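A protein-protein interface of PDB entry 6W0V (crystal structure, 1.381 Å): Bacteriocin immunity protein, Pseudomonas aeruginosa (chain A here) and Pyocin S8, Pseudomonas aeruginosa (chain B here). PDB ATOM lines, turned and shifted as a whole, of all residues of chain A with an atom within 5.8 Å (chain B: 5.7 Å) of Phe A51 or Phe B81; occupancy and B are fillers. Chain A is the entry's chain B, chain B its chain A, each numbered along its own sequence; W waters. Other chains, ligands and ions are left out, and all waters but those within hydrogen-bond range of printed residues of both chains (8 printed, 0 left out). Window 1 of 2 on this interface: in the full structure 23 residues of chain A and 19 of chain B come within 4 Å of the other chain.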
ATOM      1  N   LEU A  19      19.094 -31.701   4.038  1.00  0.00           N
ATOM      2  CA  LEU A  19      19.298 -30.760   2.910  1.00  0.00           C
ATOM      3  C   LEU A  19      19.432 -29.329   3.425  1.00  0.00           C
ATOM      4  O   LEU A  19      20.153 -28.554   2.803  1.00  0.00           O
ATOM      5  CB  LEU A  19      18.161 -30.900   1.905  1.00  0.00           C
ATOM      6  CG  LEU A  19      18.039 -32.285   1.281  1.00  0.00           C
ATOM      7  CD1 LEU A  19      16.887 -32.328   0.303  1.00  0.00           C
ATOM      8  CD2 LEU A  19      19.341 -32.686   0.597  1.00  0.00           C
ATOM      9  N   ARG A  30      24.619 -35.690  -1.743  1.00  0.00           N
ATOM     10  CA  ARG A  30      23.395 -34.896  -1.531  1.00  0.00           C
ATOM     11  C   ARG A  30      22.294 -35.464  -2.408  1.00  0.00           C
ATOM     12  O   ARG A  30      21.156 -35.553  -1.952  1.00  0.00           O
ATOM     13  CB  ARG A  30      23.595 -33.428  -1.858  1.00  0.00           C
ATOM     14  CG  ARG A  30      22.317 -32.639  -1.654  1.00  0.00           C
ATOM     15  CD  ARG A  30      22.447 -31.188  -1.979  1.00  0.00           C
ATOM     16  NE  ARG A  30      22.858 -31.025  -3.352  1.00  0.00           N
ATOM     17  CZ  ARG A  30      22.979 -29.871  -3.962  1.00  0.00           C
ATOM     18  NH1 ARG A  30      23.399 -29.853  -5.214  1.00  0.00           N
ATOM     19  NH2 ARG A  30      22.692 -28.749  -3.332  1.00  0.00           N
ATOM     20  N   ASP A  31      22.603 -35.854  -3.628  1.00  0.00           N
ATOM     21  CA  ASP A  31      21.581 -36.353  -4.571  1.00  0.00           C
ATOM     22  C   ASP A  31      20.890 -37.567  -3.973  1.00  0.00           C
ATOM     23  O   ASP A  31      19.686 -37.719  -4.194  1.00  0.00           O
ATOM     24  CB  ASP A  31      22.201 -36.753  -5.902  1.00  0.00           C
ATOM     25  CG  ASP A  31      22.335 -35.593  -6.855  1.00  0.00           C
ATOM     26  OD1 ASP A  31      21.880 -34.496  -6.495  1.00  0.00           O
ATOM     27  OD2 ASP A  31      22.888 -35.815  -7.946  1.00  0.00           O
ATOM     28  N   VAL A  34      18.342 -36.091  -1.731  1.00  0.00           N
ATOM     29  CA  VAL A  34      17.321 -35.356  -2.513  1.00  0.00           C
ATOM     30  C   VAL A  34      16.404 -36.373  -3.173  1.00  0.00           C
ATOM     31  O   VAL A  34      15.193 -36.241  -3.070  1.00  0.00           O
ATOM     32  CB  VAL A  34      17.958 -34.438  -3.563  1.00  0.00           C
ATOM     33  CG1 VAL A  34      16.916 -33.949  -4.559  1.00  0.00           C
ATOM     34  CG2 VAL A  34      18.681 -33.281  -2.901  1.00  0.00           C
ATOM     35  N   TYR A  35      16.969 -37.360  -3.843  1.00  0.00           N
ATOM     36  CA  TYR A  35      16.158 -38.306  -4.634  1.00  0.00           C
ATOM     37  C   TYR A  35      15.461 -39.299  -3.723  1.00  0.00           C
ATOM     38  O   TYR A  35      14.385 -39.738  -4.113  1.00  0.00           O
ATOM     39  CB  TYR A  35      16.984 -38.916  -5.754  1.00  0.00           C
ATOM     40  CG  TYR A  35      17.006 -37.887  -6.839  1.00  0.00           C
ATOM     41  CD1 TYR A  35      15.888 -37.703  -7.634  1.00  0.00           C
ATOM     42  CD2 TYR A  35      18.018 -36.957  -6.907  1.00  0.00           C
ATOM     43  CE1 TYR A  35      15.841 -36.692  -8.577  1.00  0.00           C
ATOM     44  CE2 TYR A  35      17.997 -35.950  -7.854  1.00  0.00           C
ATOM     45  CZ  TYR A  35      16.907 -35.818  -8.694  1.00  0.00           C
ATOM     46  OH  TYR A  35      16.853 -34.824  -9.628  1.00  0.00           O
ATOM     47  N   THR A  47      11.865 -31.903  -7.297  1.00  0.00           N
ATOM     48  CA  THR A  47      12.854 -31.247  -6.427  1.00  0.00           C
ATOM     49  C   THR A  47      12.401 -29.834  -6.084  1.00  0.00           C
ATOM     50  O   THR A  47      12.923 -29.290  -5.113  1.00  0.00           O
ATOM     51  CB  THR A  47      14.224 -31.230  -7.101  1.00  0.00           C
ATOM     52  OG1 THR A  47      14.063 -30.651  -8.396  1.00  0.00           O
ATOM     53  CG2 THR A  47      14.817 -32.616  -7.217  1.00  0.00           C
ATOM     54  N   ASP A  48      11.474 -29.259  -6.847  1.00  0.00           N
ATOM     55  CA  ASP A  48      11.027 -27.871  -6.593  1.00  0.00           C
ATOM     56  C   ASP A  48      10.458 -27.790  -5.186  1.00  0.00           C
ATOM     57  O   ASP A  48      10.574 -26.750  -4.569  1.00  0.00           O
ATOM     58  CB  ASP A  48       9.950 -27.421  -7.566  1.00  0.00           C
ATOM     59  CG  ASP A  48      10.487 -27.163  -8.951  1.00  0.00           C
ATOM     60  OD1 ASP A  48      11.695 -27.405  -9.159  1.00  0.00           O
ATOM     61  OD2 ASP A  48       9.704 -26.734  -9.791  1.00  0.00           O
ATOM     62  N   ILE A  49       9.861 -28.878  -4.727  1.00  0.00           N
ATOM     63  CA  ILE A  49       9.173 -28.893  -3.413  1.00  0.00           C
ATOM     64  C   ILE A  49      10.215 -28.633  -2.318  1.00  0.00           C
ATOM     65  O   ILE A  49       9.862 -28.090  -1.272  1.00  0.00           O
ATOM     66  CB  ILE A  49       8.416 -30.222  -3.268  1.00  0.00           C
ATOM     67  CG1 ILE A  49       7.096 -30.022  -2.526  1.00  0.00           C
ATOM     68  CG2 ILE A  49       9.302 -31.300  -2.672  1.00  0.00           C
ATOM     69  CD1 ILE A  49       6.086 -29.237  -3.340  1.00  0.00           C
ATOM     70  N   ILE A  50      11.484 -28.956  -2.579  1.00  0.00           N
ATOM     71  CA  ILE A  50      12.601 -28.691  -1.640  1.00  0.00           C
ATOM     72  C   ILE A  50      13.264 -27.374  -2.024  1.00  0.00           C
ATOM     73  O   ILE A  50      13.470 -26.529  -1.158  1.00  0.00           O
ATOM     74  CB  ILE A  50      13.624 -29.834  -1.697  1.00  0.00           C
ATOM     75  CG1 ILE A  50      12.973 -31.182  -1.374  1.00  0.00           C
ATOM     76  CG2 ILE A  50      14.793 -29.526  -0.783  1.00  0.00           C
ATOM     77  CD1 ILE A  50      13.798 -32.363  -1.804  1.00  0.00           C
ATOM     78  N   PHE A  51      13.659 -27.256  -3.288  1.00  0.00           N
ATOM     79  CA  PHE A  51      14.632 -26.229  -3.721  1.00  0.00           C
ATOM     80  C   PHE A  51      13.961 -24.950  -4.192  1.00  0.00           C
ATOM     81  O   PHE A  51      14.623 -23.926  -4.213  1.00  0.00           O
ATOM     82  CB  PHE A  51      15.533 -26.805  -4.803  1.00  0.00           C
ATOM     83  CG  PHE A  51      16.468 -27.819  -4.223  1.00  0.00           C
ATOM     84  CD1 PHE A  51      17.653 -27.420  -3.628  1.00  0.00           C
ATOM     85  CD2 PHE A  51      16.137 -29.159  -4.209  1.00  0.00           C
ATOM     86  CE1 PHE A  51      18.486 -28.354  -3.038  1.00  0.00           C
ATOM     87  CE2 PHE A  51      16.984 -30.092  -3.640  1.00  0.00           C
ATOM     88  CZ  PHE A  51      18.155 -29.684  -3.051  1.00  0.00           C
ATOM     89  N   TYR A  52      12.684 -25.009  -4.551  1.00  0.00           N
ATOM     90  CA  TYR A  52      11.946 -23.842  -5.081  1.00  0.00           C
ATOM     91  C   TYR A  52      10.634 -23.712  -4.341  1.00  0.00           C
ATOM     92  O   TYR A  52       9.577 -23.712  -4.956  1.00  0.00           O
ATOM     93  CB  TYR A  52      11.797 -23.968  -6.591  1.00  0.00           C
ATOM     94  CG  TYR A  52      13.138 -23.820  -7.236  1.00  0.00           C
ATOM     95  CD1 TYR A  52      13.623 -22.562  -7.525  1.00  0.00           C
ATOM     96  CD2 TYR A  52      13.962 -24.914  -7.411  1.00  0.00           C
ATOM     97  CE1 TYR A  52      14.882 -22.389  -8.055  1.00  0.00           C
ATOM     98  CE2 TYR A  52      15.227 -24.759  -7.940  1.00  0.00           C
ATOM     99  CZ  TYR A  52      15.681 -23.496  -8.256  1.00  0.00           C
ATOM    100  OH  TYR A  52      16.917 -23.334  -8.787  1.00  0.00           O
ATOM    101  N   PRO A  53      10.686 -23.513  -3.014  1.00  0.00           N
ATOM    102  CA  PRO A  53       9.474 -23.154  -2.286  1.00  0.00           C
ATOM    103  C   PRO A  53       8.969 -21.851  -2.922  1.00  0.00           C
ATOM    104  O   PRO A  53       9.789 -20.995  -3.223  1.00  0.00           O
ATOM    105  CB  PRO A  53       9.962 -22.978  -0.844  1.00  0.00           C
ATOM    106  CG  PRO A  53      11.429 -22.630  -0.994  1.00  0.00           C
ATOM    107  CD  PRO A  53      11.889 -23.461  -2.173  1.00  0.00           C
ATOM    108  N   ARG B  67      16.964 -20.386  -2.730  1.00  0.00           N
ATOM    109  CA  ARG B  67      16.287 -20.719  -1.469  1.00  0.00           C
ATOM    110  C   ARG B  67      17.253 -21.547  -0.629  1.00  0.00           C
ATOM    111  O   ARG B  67      18.406 -21.730  -1.006  1.00  0.00           O
ATOM    112  CB  ARG B  67      14.917 -21.325  -1.775  1.00  0.00           C
ATOM    113  CG  ARG B  67      14.036 -20.411  -2.620  1.00  0.00           C
ATOM    114  CD  ARG B  67      13.429 -19.249  -1.854  1.00  0.00           C
ATOM    115  NE  ARG B  67      14.399 -18.406  -1.175  1.00  0.00           N
ATOM    116  CZ  ARG B  67      15.085 -17.410  -1.732  1.00  0.00           C
ATOM    117  NH1 ARG B  67      14.929 -17.105  -3.010  1.00  0.00           N
ATOM    118  NH2 ARG B  67      15.938 -16.719  -0.994  1.00  0.00           N
ATOM    119  N   LYS B  68      16.829 -21.967   0.546  1.00  0.00           N
ATOM    120  CA  LYS B  68      17.769 -22.329   1.624  1.00  0.00           C
ATOM    121  C   LYS B  68      18.544 -23.591   1.258  1.00  0.00           C
ATOM    122  O   LYS B  68      19.738 -23.608   1.519  1.00  0.00           O
ATOM    123  CB  LYS B  68      17.010 -22.471   2.938  1.00  0.00           C
ATOM    124  CG  LYS B  68      16.773 -21.130   3.597  1.00  0.00           C
ATOM    125  CD  LYS B  68      15.943 -21.197   4.842  1.00  0.00           C
ATOM    126  CE  LYS B  68      15.721 -19.827   5.444  1.00  0.00           C
ATOM    127  NZ  LYS B  68      15.238 -19.923   6.838  1.00  0.00           N
ATOM    128  N   THR B  69      17.900 -24.621   0.719  1.00  0.00           N
ATOM    129  CA  THR B  69      18.635 -25.873   0.408  1.00  0.00           C
ATOM    130  C   THR B  69      19.623 -25.578  -0.712  1.00  0.00           C
ATOM    131  O   THR B  69      20.759 -26.017  -0.591  1.00  0.00           O
ATOM    132  CB  THR B  69      17.701 -27.050   0.129  1.00  0.00           C
ATOM    133  OG1 THR B  69      16.790 -26.681  -0.898  1.00  0.00           O
ATOM    134  CG2 THR B  69      16.973 -27.468   1.382  1.00  0.00           C
ATOM    135  N   ASN B  70      19.218 -24.832  -1.738  1.00  0.00           N
ATOM    136  CA  ASN B  70      20.183 -24.486  -2.813  1.00  0.00           C
ATOM    137  C   ASN B  70      21.341 -23.721  -2.198  1.00  0.00           C
ATOM    138  O   ASN B  70      22.494 -24.076  -2.482  1.00  0.00           O
ATOM    139  CB  ASN B  70      19.534 -23.709  -3.950  1.00  0.00           C
ATOM    140  CG  ASN B  70      19.197 -24.645  -5.083  1.00  0.00           C
ATOM    141  OD1 ASN B  70      19.749 -25.742  -5.147  1.00  0.00           O
ATOM    142  ND2 ASN B  70      18.292 -24.238  -5.952  1.00  0.00           N
ATOM    143  N   SER B  79      26.427 -27.637  -6.730  1.00  0.00           N
ATOM    144  CA  SER B  79      25.654 -26.962  -7.787  1.00  0.00           C
ATOM    145  C   SER B  79      24.215 -26.904  -7.330  1.00  0.00           C
ATOM    146  O   SER B  79      23.666 -27.908  -6.908  1.00  0.00           O
ATOM    147  CB  SER B  79      25.770 -27.672  -9.072  1.00  0.00           C
ATOM    148  OG  SER B  79      27.136 -27.823  -9.396  1.00  0.00           O
ATOM    149  N   PRO B  80      23.596 -25.723  -7.392  1.00  0.00           N
ATOM    150  CA  PRO B  80      22.190 -25.621  -7.051  1.00  0.00           C
ATOM    151  C   PRO B  80      21.362 -26.394  -8.076  1.00  0.00           C
ATOM    152  O   PRO B  80      21.655 -26.443  -9.249  1.00  0.00           O
ATOM    153  CB  PRO B  80      21.881 -24.131  -7.084  1.00  0.00           C
ATOM    154  CG  PRO B  80      22.942 -23.553  -7.986  1.00  0.00           C
ATOM    155  CD  PRO B  80      24.156 -24.441  -7.817  1.00  0.00           C
ATOM    156  N   PHE B  81      20.295 -26.995  -7.591  1.00  0.00           N
ATOM    157  CA  PHE B  81      19.274 -27.585  -8.460  1.00  0.00           C
ATOM    158  C   PHE B  81      18.582 -26.469  -9.208  1.00  0.00           C
ATOM    159  O   PHE B  81      18.323 -25.398  -8.631  1.00  0.00           O
ATOM    160  CB  PHE B  81      18.251 -28.320  -7.614  1.00  0.00           C
ATOM    161  CG  PHE B  81      18.749 -29.644  -7.131  1.00  0.00           C
ATOM    162  CD1 PHE B  81      19.596 -29.726  -6.044  1.00  0.00           C
ATOM    163  CD2 PHE B  81      18.403 -30.804  -7.799  1.00  0.00           C
ATOM    164  CE1 PHE B  81      20.065 -30.955  -5.615  1.00  0.00           C
ATOM    165  CE2 PHE B  81      18.876 -32.030  -7.368  1.00  0.00           C
ATOM    166  CZ  PHE B  81      19.713 -32.100  -6.282  1.00  0.00           C
ATOM    167  N   THR B  82      18.253 -26.748 -10.452  1.00  0.00           N
ATOM    168  CA  THR B  82      17.386 -25.867 -11.244  1.00  0.00           C
ATOM    169  C   THR B  82      15.965 -26.216 -10.875  1.00  0.00           C
ATOM    170  O   THR B  82      15.702 -27.293 -10.332  1.00  0.00           O
ATOM    171  CB  THR B  82      17.581 -26.047 -12.747  1.00  0.00           C
ATOM    172  OG1 THR B  82      17.040 -27.296 -13.151  1.00  0.00           O
ATOM    173  CG2 THR B  82      19.036 -26.009 -13.136  1.00  0.00           C
ATOM    174  N   PRO B  83      15.011 -25.343 -11.224  1.00  0.00           N
ATOM    175  CA  PRO B  83      13.616 -25.743 -11.178  1.00  0.00           C
ATOM    176  C   PRO B  83      13.492 -27.016 -12.012  1.00  0.00           C
ATOM    177  O   PRO B  83      14.212 -27.211 -12.981  1.00  0.00           O
ATOM    178  CB  PRO B  83      12.859 -24.566 -11.784  1.00  0.00           C
ATOM    179  CG  PRO B  83      13.788 -23.399 -11.555  1.00  0.00           C
ATOM    180  CD  PRO B  83      15.189 -23.963 -11.694  1.00  0.00           C
ATOM    181  N   GLN B  87      15.274 -29.039 -15.661  1.00  0.00           N
ATOM    182  CA  GLN B  87      16.097 -30.260 -15.534  1.00  0.00           C
ATOM    183  C   GLN B  87      15.944 -31.083 -16.806  1.00  0.00           C
ATOM    184  O   GLN B  87      14.902 -30.989 -17.474  1.00  0.00           O
ATOM    185  CB  GLN B  87      15.688 -31.038 -14.295  1.00  0.00           C
ATOM    186  CG  GLN B  87      15.719 -30.149 -13.067  1.00  0.00           C
ATOM    187  CD  GLN B  87      15.328 -30.839 -11.789  1.00  0.00           C
ATOM    188  OE1 GLN B  87      15.440 -30.254 -10.714  1.00  0.00           O
ATOM    189  NE2 GLN B  87      14.897 -32.082 -11.905  1.00  0.00           N
ATOM    190  N   ASP B  92      20.090 -32.121 -13.220  1.00  0.00           N
ATOM    191  CA  ASP B  92      19.106 -31.311 -12.468  1.00  0.00           C
ATOM    192  C   ASP B  92      19.769 -30.111 -11.803  1.00  0.00           C
ATOM    193  O   ASP B  92      19.074 -29.359 -11.116  1.00  0.00           O
ATOM    194  CB  ASP B  92      18.423 -32.179 -11.416  1.00  0.00           C
ATOM    195  CG  ASP B  92      19.394 -32.983 -10.575  1.00  0.00           C
ATOM    196  OD1 ASP B  92      20.586 -32.637 -10.570  1.00  0.00           O
ATOM    197  OD2 ASP B  92      18.949 -33.953  -9.946  1.00  0.00           O
ATOM    198  N   LYS B  93      21.067 -29.924 -12.020  1.00  0.00           N
ATOM    199  CA  LYS B  93      21.839 -28.831 -11.402  1.00  0.00           C
ATOM    200  C   LYS B  93      22.102 -27.775 -12.458  1.00  0.00           C
ATOM    201  O   LYS B  93      22.242 -28.130 -13.641  1.00  0.00           O
ATOM    202  CB  LYS B  93      23.223 -29.279 -10.946  1.00  0.00           C
ATOM    203  CG  LYS B  93      23.274 -30.568 -10.167  1.00  0.00           C
ATOM    204  CD  LYS B  93      22.425 -30.480  -8.942  1.00  0.00           C
ATOM    205  CE  LYS B  93      22.701 -31.635  -8.012  1.00  0.00           C
ATOM    206  NZ  LYS B  93      22.488 -32.935  -8.688  1.00  0.00           N
ATOM    207  N   TYR B  94      22.242 -26.539 -12.029  1.00  0.00           N
ATOM    208  CA  TYR B  94      22.824 -25.494 -12.890  1.00  0.00           C
ATOM    209  C   TYR B  94      24.171 -25.997 -13.371  1.00  0.00           C
ATOM    210  O   TYR B  94      24.975 -26.460 -12.566  1.00  0.00           O
ATOM    211  CB  TYR B  94      22.921 -24.177 -12.145  1.00  0.00           C
ATOM    212  CG  TYR B  94      21.587 -23.506 -12.103  1.00  0.00           C
ATOM    213  CD1 TYR B  94      21.065 -22.918 -13.237  1.00  0.00           C
ATOM    214  CD2 TYR B  94      20.811 -23.550 -10.961  1.00  0.00           C
ATOM    215  CE1 TYR B  94      19.825 -22.315 -13.225  1.00  0.00           C
ATOM    216  CE2 TYR B  94      19.573 -22.946 -10.928  1.00  0.00           C
ATOM    217  CZ  TYR B  94      19.079 -22.333 -12.062  1.00  0.00           C
ATOM    218  OH  TYR B  94      17.861 -21.739 -12.051  1.00  0.00           O
HETATM  219  O   HOH W   1      15.128 -24.568  -0.116  1.00  0.00           O
HETATM  220  O   HOH W   2      12.633 -32.987  -9.850  1.00  0.00           O
HETATM  221  O   HOH W   3      16.627 -23.939  -2.366  1.00  0.00           O
HETATM  222  O   HOH W   4      14.064 -28.095  -8.286  1.00  0.00           O
HETATM  223  O   HOH W   5      21.354 -28.537  -0.958  1.00  0.00           O
HETATM  224  O   HOH W   6      17.311 -20.689  -9.788  1.00  0.00           O
HETATM  225  O   HOH W   7      23.316 -26.193  -4.104  1.00  0.00           O
HETATM  226  O   HOH W   8      16.459 -22.084  -5.046  1.00  0.00           O
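OG1 of Thr B69 sits at hydrogen-bond distance from O of Ile A50 (3.3 Å). The side-chain hydroxyl of Tyr A52 sits at hydrogen-bond distance from the side-chain amide nitrogen of Asn B70. O of Ser B79 lies within hydrogen-bond range of NH1 of Arg A30 (2.6 Å). The side-chain hydroxyl (OH) of Tyr A52 sits at hydrogen-bond distance from the backbone carbonyl oxygen (O) of Phe B81 (2.5 Å). The side-chain amide oxygen of Gln B87 sits at hydrogen-bond distance from the side-chain hydroxyl of Thr A47. The side-chain amino group of Lys B93 is in salt-bridge range of the side-chain carboxylate of Asp A31 (2.8 Å). The side-chain hydroxyl of Tyr A35 lies close to the side-chain carboxylate of Asp B92 (2.3 Å).
Water W6 lies within hydrogen-bond range of the side-chain hydroxyl (OH) of Tyr B94 (2.6 Å) and the side-chain hydroxyl (OH) of Tyr A52 (2.9 Å). Water W4 lies within hydrogen-bond range of OG1 of Thr A47 (2.6 Å), OD1 of Asp A48 (2.6 Å) and O of Thr B82 (2.7 Å). Water W5 bridges the backbone carbonyl oxygen of Thr B69 (2.6 Å) and the guanidinium group of Arg A30 (2.7 Å). Water W3 lies within hydrogen-bond range of the backbone carbonyl oxygen (O) of Phe A51 (2.7 Å), the backbone NH (N) of Asn B70 (2.8 Å), the side-chain hydroxyl (OG1) of Thr B69 (3.1 Å) and the backbone carbonyl oxygen (O) of Arg B67 (3.1 Å). Water W8 lies within hydrogen-bond range of the backbone carbonyl oxygen of Phe A51 (2.7 Å), the backbone NH of Arg B67 (2.9 Å) and the side-chain amide nitrogen of Asn B70 (3.0 Å). Water W2 bridges N of Thr A47 and NE2 of Gln B87.
N of Phe B81 is in hydrogen-bond range of OD1 of Asn B70. O of Pro B80 is in hydrogen-bond range of N of Tyr B94 (2.8 Å). The backbone carbonyl oxygen (O) of Thr B82 lies close to the side-chain amide oxygen (OE1) of Gln B87. The backbone NH (N) of Thr B82 sits at hydrogen-bond distance from the backbone carbonyl oxygen (O) of Asp B92, 2.8 Å away. OD1 of Asp B92 lies within salt-bridge range of NZ of Lys B93 (2.7 Å).
Ile A49 touches none of the printed residues of chain B. Of the printed residues of chain B, Phe A51 touches Arg B67 (3.6 Å), Thr B69 (3.0 Å), Asn B70 (3.1 Å) and Phe B81 (3.3 Å). Printed residues of chain A within 4 Å of Ser B79: Arg A30. Pro B80 touches none of the printed residues of chain A. Of chain A, only Arg A30 (3.5 Å), Asp A31 (3.2 Å), Val A34 (3.7 Å), Phe A51 (3.3 Å) and Tyr A52 (2.5 Å) come within 4 Å of Phe B81. Of the printed residues of chain A, Pro B83 touches Asp A48 and Tyr A52.
Leu A19 touches Thr B69. NH1 of Arg A30 touches CE of Lys B93 (3.4 Å). Asp A31 touches Phe B81 (OD1 to CZ, 3.2 Å). CZ of Phe B81 touches CG2 of Val A34, 3.7 Å away. CD1 of Phe A51 touches OG1 of Thr B69, 3.0 Å away. Phe B81 touches Phe A51. Tyr A52 touches Thr B82. Pro B83 touches Tyr A52 (N to CE2, 3.3 Å). Tyr A52 touches Tyr B94 (OH to CE2, 3.4 Å). Pro A53 touches Arg B67 (CD to CB, 3.7 Å).
Hydrophobic or aromatic side chains of chain A within 4 Å of the printed part of chain B: Leu A19, Val A34, Tyr A35, Ile A50, Phe A51, Tyr A52 and Pro A53. Among the printed residues, 21 pairs touch across the chains. Among the printed residues, Asp or Glu carboxylates within 4 Å of a Lys or Arg side-chain nitrogen of the other chain: Asp A31 with Lys B93.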
